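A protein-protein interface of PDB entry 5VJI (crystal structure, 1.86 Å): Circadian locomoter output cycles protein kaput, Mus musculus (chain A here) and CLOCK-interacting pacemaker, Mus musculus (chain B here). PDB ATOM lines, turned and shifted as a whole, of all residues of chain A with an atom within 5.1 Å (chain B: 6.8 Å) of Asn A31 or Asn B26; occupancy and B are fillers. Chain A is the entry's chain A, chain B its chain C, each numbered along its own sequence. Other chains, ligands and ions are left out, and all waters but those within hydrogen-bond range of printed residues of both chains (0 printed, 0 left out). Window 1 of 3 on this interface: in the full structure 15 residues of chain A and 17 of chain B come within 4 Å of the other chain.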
ATOM      1  N   MET A  27      28.142 -30.461 -28.058  1.00  0.00           N
ATOM      2  CA  MET A  27      27.575 -29.101 -28.081  1.00  0.00           C
ATOM      3  C   MET A  27      27.129 -28.611 -26.674  1.00  0.00           C
ATOM      4  O   MET A  27      27.389 -27.457 -26.278  1.00  0.00           O
ATOM      5  CB  MET A  27      26.362 -29.057 -29.026  1.00  0.00           C
ATOM      6  CG  MET A  27      26.295 -27.929 -30.023  1.00  0.00           C
ATOM      7  SD  MET A  27      24.965 -28.358 -31.464  1.00  0.00           S
ATOM      8  CE  MET A  27      25.848 -29.914 -32.252  1.00  0.00           C
ATOM      9  N   ILE A  28      26.400 -29.488 -25.986  1.00  0.00           N
ATOM     10  CA  ILE A  28      25.994 -29.257 -24.594  1.00  0.00           C
ATOM     11  C   ILE A  28      27.226 -29.034 -23.728  1.00  0.00           C
ATOM     12  O   ILE A  28      27.290 -28.062 -22.974  1.00  0.00           O
ATOM     13  CB  ILE A  28      25.162 -30.430 -24.040  1.00  0.00           C
ATOM     14  CG1 ILE A  28      23.859 -30.616 -24.825  1.00  0.00           C
ATOM     15  CG2 ILE A  28      24.853 -30.200 -22.472  1.00  0.00           C
ATOM     16  CD1 ILE A  28      23.169 -32.014 -24.524  1.00  0.00           C
ATOM     17  N   GLU A  29      28.243 -29.900 -23.881  1.00  0.00           N
ATOM     18  CA  GLU A  29      29.442 -29.771 -23.050  1.00  0.00           C
ATOM     19  C   GLU A  29      30.087 -28.396 -23.239  1.00  0.00           C
ATOM     20  O   GLU A  29      30.450 -27.741 -22.258  1.00  0.00           O
ATOM     21  CB  GLU A  29      30.437 -30.892 -23.387  1.00  0.00           C
ATOM     22  CG  GLU A  29      31.601 -31.002 -22.378  1.00  0.00           C
ATOM     23  CD  GLU A  29      32.376 -32.293 -22.603  1.00  0.00           C
ATOM     24  OE1 GLU A  29      31.967 -33.080 -23.499  1.00  0.00           O
ATOM     25  OE2 GLU A  29      33.385 -32.537 -21.909  1.00  0.00           O
ATOM     26  N   ALA A  30      30.187 -27.932 -24.489  1.00  0.00           N
ATOM     27  CA  ALA A  30      30.812 -26.640 -24.809  1.00  0.00           C
ATOM     28  C   ALA A  30      29.956 -25.477 -24.313  1.00  0.00           C
ATOM     29  O   ALA A  30      30.503 -24.501 -23.802  1.00  0.00           O
ATOM     30  CB  ALA A  30      31.087 -26.513 -26.309  1.00  0.00           C
ATOM     31  N   ASN A  31      28.628 -25.566 -24.426  1.00  0.00           N
ATOM     32  CA  ASN A  31      27.738 -24.541 -23.884  1.00  0.00           C
ATOM     33  C   ASN A  31      27.843 -24.428 -22.380  1.00  0.00           C
ATOM     34  O   ASN A  31      27.777 -23.318 -21.832  1.00  0.00           O
ATOM     35  CB  ASN A  31      26.284 -24.858 -24.182  1.00  0.00           C
ATOM     36  CG  ASN A  31      25.816 -24.302 -25.472  1.00  0.00           C
ATOM     37  OD1 ASN A  31      26.102 -23.152 -25.809  1.00  0.00           O
ATOM     38  ND2 ASN A  31      25.009 -25.085 -26.183  1.00  0.00           N
ATOM     39  N   ILE A  32      27.913 -25.574 -21.689  1.00  0.00           N
ATOM     40  CA  ILE A  32      28.066 -25.539 -20.237  1.00  0.00           C
ATOM     41  C   ILE A  32      29.338 -24.786 -19.875  1.00  0.00           C
ATOM     42  O   ILE A  32      29.363 -23.984 -18.932  1.00  0.00           O
ATOM     43  CB  ILE A  32      28.064 -26.971 -19.663  1.00  0.00           C
ATOM     44  CG1 ILE A  32      26.629 -27.531 -19.633  1.00  0.00           C
ATOM     45  CG2 ILE A  32      28.777 -27.018 -18.281  1.00  0.00           C
ATOM     46  CD1 ILE A  32      26.570 -28.965 -19.164  1.00  0.00           C
ATOM     47  N   HIS A  33      30.426 -25.057 -20.588  1.00  0.00           N
ATOM     48  CA  HIS A  33      31.663 -24.344 -20.283  1.00  0.00           C
ATOM     49  C   HIS A  33      31.505 -22.846 -20.522  1.00  0.00           C
ATOM     50  O   HIS A  33      32.028 -22.045 -19.745  1.00  0.00           O
ATOM     51  CB  HIS A  33      32.807 -24.923 -21.112  1.00  0.00           C
ATOM     52  CG  HIS A  33      33.305 -26.229 -20.594  1.00  0.00           C
ATOM     53  ND1 HIS A  33      33.509 -27.325 -21.405  1.00  0.00           N
ATOM     54  CD2 HIS A  33      33.630 -26.619 -19.338  1.00  0.00           C
ATOM     55  CE1 HIS A  33      33.938 -28.335 -20.670  1.00  0.00           C
ATOM     56  NE2 HIS A  33      34.023 -27.931 -19.415  1.00  0.00           N
ATOM     57  N   ARG A  34      30.821 -22.457 -21.609  1.00  0.00           N
ATOM     58  CA  ARG A  34      30.607 -21.035 -21.872  1.00  0.00           C
ATOM     59  C   ARG A  34      29.723 -20.404 -20.806  1.00  0.00           C
ATOM     60  O   ARG A  34      29.971 -19.263 -20.391  1.00  0.00           O
ATOM     61  CB  ARG A  34      29.994 -20.858 -23.264  1.00  0.00           C
ATOM     62  CG  ARG A  34      29.967 -19.440 -23.788  1.00  0.00           C
ATOM     63  CD  ARG A  34      29.380 -19.369 -25.204  1.00  0.00           C
ATOM     64  NE  ARG A  34      28.159 -20.166 -25.354  1.00  0.00           N
ATOM     65  CZ  ARG A  34      26.984 -19.924 -24.769  1.00  0.00           C
ATOM     66  NH1 ARG A  34      26.826 -18.903 -23.945  1.00  0.00           N
ATOM     67  NH2 ARG A  34      25.963 -20.748 -24.988  1.00  0.00           N
ATOM     68  N   GLN A  35      28.677 -21.117 -20.357  1.00  0.00           N
ATOM     69  CA  GLN A  35      27.791 -20.557 -19.335  1.00  0.00           C
ATOM     70  C   GLN A  35      28.525 -20.405 -18.010  1.00  0.00           C
ATOM     71  O   GLN A  35      28.308 -19.449 -17.270  1.00  0.00           O
ATOM     72  CB  GLN A  35      26.566 -21.469 -19.154  1.00  0.00           C
ATOM     73  CG  GLN A  35      25.638 -21.463 -20.367  1.00  0.00           C
ATOM     74  CD  GLN A  35      24.680 -22.644 -20.294  1.00  0.00           C
ATOM     75  OE1 GLN A  35      24.939 -23.619 -19.579  1.00  0.00           O
ATOM     76  NE2 GLN A  35      23.584 -22.568 -21.031  1.00  0.00           N
ATOM     77  N   GLN A  36      29.414 -21.334 -17.699  1.00  0.00           N
ATOM     78  CA  GLN A  36      30.252 -21.151 -16.516  1.00  0.00           C
ATOM     79  C   GLN A  36      31.111 -19.895 -16.608  1.00  0.00           C
ATOM     80  O   GLN A  36      31.290 -19.191 -15.606  1.00  0.00           O
ATOM     81  CB  GLN A  36      31.132 -22.389 -16.299  1.00  0.00           C
ATOM     82  CG  GLN A  36      30.414 -23.448 -15.467  1.00  0.00           C
ATOM     83  CD  GLN A  36      31.037 -24.848 -15.539  1.00  0.00           C
ATOM     84  OE1 GLN A  36      32.006 -25.101 -16.277  1.00  0.00           O
ATOM     85  NE2 GLN A  36      30.445 -25.778 -14.803  1.00  0.00           N
ATOM     86  N   GLU B  21      15.844 -33.869 -23.010  1.00  0.00           N
ATOM     87  CA  GLU B  21      15.576 -33.218 -21.711  1.00  0.00           C
ATOM     88  C   GLU B  21      16.782 -32.405 -21.223  1.00  0.00           C
ATOM     89  O   GLU B  21      16.604 -31.336 -20.639  1.00  0.00           O
ATOM     90  CB  GLU B  21      15.150 -34.255 -20.683  1.00  0.00           C
ATOM     91  CG  GLU B  21      15.210 -33.778 -19.205  1.00  0.00           C
ATOM     92  CD  GLU B  21      14.170 -32.675 -18.858  1.00  0.00           C
ATOM     93  OE1 GLU B  21      13.283 -32.372 -19.700  1.00  0.00           O
ATOM     94  OE2 GLU B  21      14.216 -32.116 -17.731  1.00  0.00           O
ATOM     95  N   LEU B  22      18.009 -32.856 -21.491  1.00  0.00           N
ATOM     96  CA  LEU B  22      19.173 -32.081 -21.066  1.00  0.00           C
ATOM     97  C   LEU B  22      19.302 -30.822 -21.883  1.00  0.00           C
ATOM     98  O   LEU B  22      19.586 -29.747 -21.337  1.00  0.00           O
ATOM     99  CB  LEU B  22      20.440 -32.912 -21.198  1.00  0.00           C
ATOM    100  CG  LEU B  22      21.788 -32.232 -20.970  1.00  0.00           C
ATOM    101  CD1 LEU B  22      21.793 -31.700 -19.528  1.00  0.00           C
ATOM    102  CD2 LEU B  22      22.886 -33.268 -21.123  1.00  0.00           C
ATOM    103  N   ILE B  23      19.007 -30.913 -23.178  1.00  0.00           N
ATOM    104  CA  ILE B  23      19.008 -29.720 -24.020  1.00  0.00           C
ATOM    105  C   ILE B  23      17.964 -28.729 -23.519  1.00  0.00           C
ATOM    106  O   ILE B  23      18.224 -27.529 -23.420  1.00  0.00           O
ATOM    107  CB  ILE B  23      18.761 -30.097 -25.488  1.00  0.00           C
ATOM    108  CG1 ILE B  23      19.929 -30.923 -26.051  1.00  0.00           C
ATOM    109  CG2 ILE B  23      18.563 -28.805 -26.294  1.00  0.00           C
ATOM    110  CD1 ILE B  23      19.664 -31.627 -27.404  1.00  0.00           C
ATOM    111  N   ARG B  24      16.756 -29.215 -23.213  1.00  0.00           N
ATOM    112  CA  ARG B  24      15.738 -28.326 -22.653  1.00  0.00           C
ATOM    113  C   ARG B  24      16.265 -27.624 -21.401  1.00  0.00           C
ATOM    114  O   ARG B  24      16.165 -26.406 -21.271  1.00  0.00           O
ATOM    115  CB  ARG B  24      14.468 -29.097 -22.306  1.00  0.00           C
ATOM    116  CG  ARG B  24      13.283 -28.163 -21.935  1.00  0.00           C
ATOM    117  CD  ARG B  24      12.181 -28.956 -21.118  1.00  0.00           C
ATOM    118  NE  ARG B  24      12.656 -29.557 -19.851  1.00  0.00           N
ATOM    119  CZ  ARG B  24      13.031 -28.879 -18.764  1.00  0.00           C
ATOM    120  NH1 ARG B  24      12.972 -27.545 -18.733  1.00  0.00           N
ATOM    121  NH2 ARG B  24      13.412 -29.551 -17.672  1.00  0.00           N
ATOM    122  N   GLN B  25      16.789 -28.393 -20.453  1.00  0.00           N
ATOM    123  CA  GLN B  25      17.301 -27.780 -19.230  1.00  0.00           C
ATOM    124  C   GLN B  25      18.378 -26.741 -19.520  1.00  0.00           C
ATOM    125  O   GLN B  25      18.423 -25.667 -18.869  1.00  0.00           O
ATOM    126  CB  GLN B  25      17.859 -28.865 -18.319  1.00  0.00           C
ATOM    127  CG  GLN B  25      16.770 -29.744 -17.724  1.00  0.00           C
ATOM    128  CD  GLN B  25      17.388 -30.780 -16.764  1.00  0.00           C
ATOM    129  OE1 GLN B  25      18.358 -30.472 -16.066  1.00  0.00           O
ATOM    130  NE2 GLN B  25      16.822 -31.994 -16.719  1.00  0.00           N
ATOM    131  N   ASN B  26      19.308 -27.072 -20.430  1.00  0.00           N
ATOM    132  CA  ASN B  26      20.417 -26.179 -20.686  1.00  0.00           C
ATOM    133  C   ASN B  26      19.953 -24.898 -21.368  1.00  0.00           C
ATOM    134  O   ASN B  26      20.494 -23.825 -21.102  1.00  0.00           O
ATOM    135  CB  ASN B  26      21.472 -26.832 -21.554  1.00  0.00           C
ATOM    136  CG  ASN B  26      22.763 -26.034 -21.533  1.00  0.00           C
ATOM    137  OD1 ASN B  26      23.118 -25.487 -22.514  1.00  0.00           O
ATOM    138  ND2 ASN B  26      23.444 -25.962 -20.371  1.00  0.00           N
ATOM    139  N   GLN B  27      18.980 -25.001 -22.277  1.00  0.00           N
ATOM    140  CA  GLN B  27      18.372 -23.797 -22.841  1.00  0.00           C
ATOM    141  C   GLN B  27      17.670 -22.949 -21.784  1.00  0.00           C
ATOM    142  O   GLN B  27      17.740 -21.714 -21.843  1.00  0.00           O
ATOM    143  CB  GLN B  27      17.386 -24.187 -23.937  1.00  0.00           C
ATOM    144  CG  GLN B  27      18.102 -24.730 -25.197  1.00  0.00           C
ATOM    145  CD  GLN B  27      17.147 -25.211 -26.316  1.00  0.00           C
ATOM    146  OE1 GLN B  27      15.943 -25.360 -26.126  1.00  0.00           O
ATOM    147  NE2 GLN B  27      17.718 -25.501 -27.469  1.00  0.00           N
ATOM    148  N   ALA B  28      16.960 -23.589 -20.841  1.00  0.00           N
ATOM    149  CA  ALA B  28      16.343 -22.870 -19.714  1.00  0.00           C
ATOM    150  C   ALA B  28      17.395 -22.125 -18.886  1.00  0.00           C
ATOM    151  O   ALA B  28      17.173 -20.983 -18.463  1.00  0.00           O
ATOM    152  CB  ALA B  28      15.552 -23.837 -18.812  1.00  0.00           C
ATOM    153  N   THR B  29      18.542 -22.755 -18.646  1.00  0.00           N
ATOM    154  CA  THR B  29      19.615 -22.126 -17.891  1.00  0.00           C
ATOM    155  C   THR B  29      20.209 -20.937 -18.655  1.00  0.00           C
ATOM    156  O   THR B  29      20.511 -19.877 -18.067  1.00  0.00           O
ATOM    157  CB  THR B  29      20.663 -23.206 -17.558  1.00  0.00           C
ATOM    158  OG1 THR B  29      20.156 -24.030 -16.481  1.00  0.00           O
ATOM    159  CG2 THR B  29      21.944 -22.590 -17.152  1.00  0.00           C
ATOM    160  N   GLN B  30      20.332 -21.063 -19.967  1.00  0.00           N
ATOM    161  CA  GLN B  30      20.812 -19.929 -20.759  1.00  0.00           C
ATOM    162  C   GLN B  30      19.852 -18.735 -20.686  1.00  0.00           C
ATOM    163  O   GLN B  30      20.297 -17.580 -20.613  1.00  0.00           O
ATOM    164  CB  GLN B  30      21.013 -20.327 -22.230  1.00  0.00           C
ATOM    165  CG  GLN B  30      21.676 -19.186 -23.062  1.00  0.00           C
ATOM    166  CD  GLN B  30      23.098 -18.913 -22.595  1.00  0.00           C
ATOM    167  OE1 GLN B  30      23.869 -19.849 -22.498  1.00  0.00           O
ATOM    168  NE2 GLN B  30      23.443 -17.632 -22.282  1.00  0.00           N
ATOM    169  N   ALA B  31      18.534 -18.987 -20.699  1.00  0.00           N
ATOM    170  CA  ALA B  31      17.577 -17.893 -20.521  1.00  0.00           C
ATOM    171  C   ALA B  31      17.710 -17.252 -19.139  1.00  0.00           C
ATOM    172  O   ALA B  31      17.637 -16.027 -19.004  1.00  0.00           O
ATOM    173  CB  ALA B  31      16.140 -18.389 -20.713  1.00  0.00           C
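The backbone carbonyl oxygen of Met A27 lies within hydrogen-bond range of the side-chain amide nitrogen of Asn A31 (3.4 Å).
The guanidinium group of Arg A34 sits at hydrogen-bond distance from the side-chain amide oxygen of Asn A31 (2.5 Å).
OG1 of Thr B29 is in hydrogen-bond range of O of Gln B25 (3.4 Å).
Hydrophobic or aromatic side chains of chain B within 4 Å of the printed part of chain A: Leu B22 and Ile B23.
Hydrophobic or aromatic side chains of chain A that line the printed part of chain B: Ile A28 and Ile A32.
Among the printed residues, no Asp or Glu carboxylate lies within 4 Å of a Lys or Arg side-chain nitrogen of the other chain.
Asn A31 touches one residue of chain B.
Of the printed residues of chain B, Ile A32 touches Asn B26.
Of the printed residues of chain B, Gln A35 touches Asn B26, Thr B29 and Gln B30.
Printed residues of chain A within 4 Å of Leu B22: Ile A28.
Asn B26 touches three residues of chain A.
The nearest residue of chain B that does not touch Asn A31 is Gln B30 (5.2 Å).
The nearest residue of chain A that does not touch Asn B26 is Ile A28 (4.8 Å).
The guanidinium group (NH2) of Arg A34 sits at hydrogen-bond distance from the side-chain amide oxygen (OE1) of Gln B30 (3.4 Å).
OE1 of Gln A35 lies within hydrogen-bond range of ND2 of Asn B26, 2.9 Å away.
NE2 of Gln A35 sits at hydrogen-bond distance from OE1 of Gln B30 (3.1 Å).
CD1 of Ile A28 touches CD2 of Leu B22 (3.6 Å).
Ile A28 touches Ile B23 (CD1 to CG1, 3.7 Å).
Asn B26 touches Asn A31.
Asn B26 touches Ile A32 (ND2 to CG1, 3.6 Å).
CG2 of Thr B29 touches OE1 of Gln A35, at 3.99 Å.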
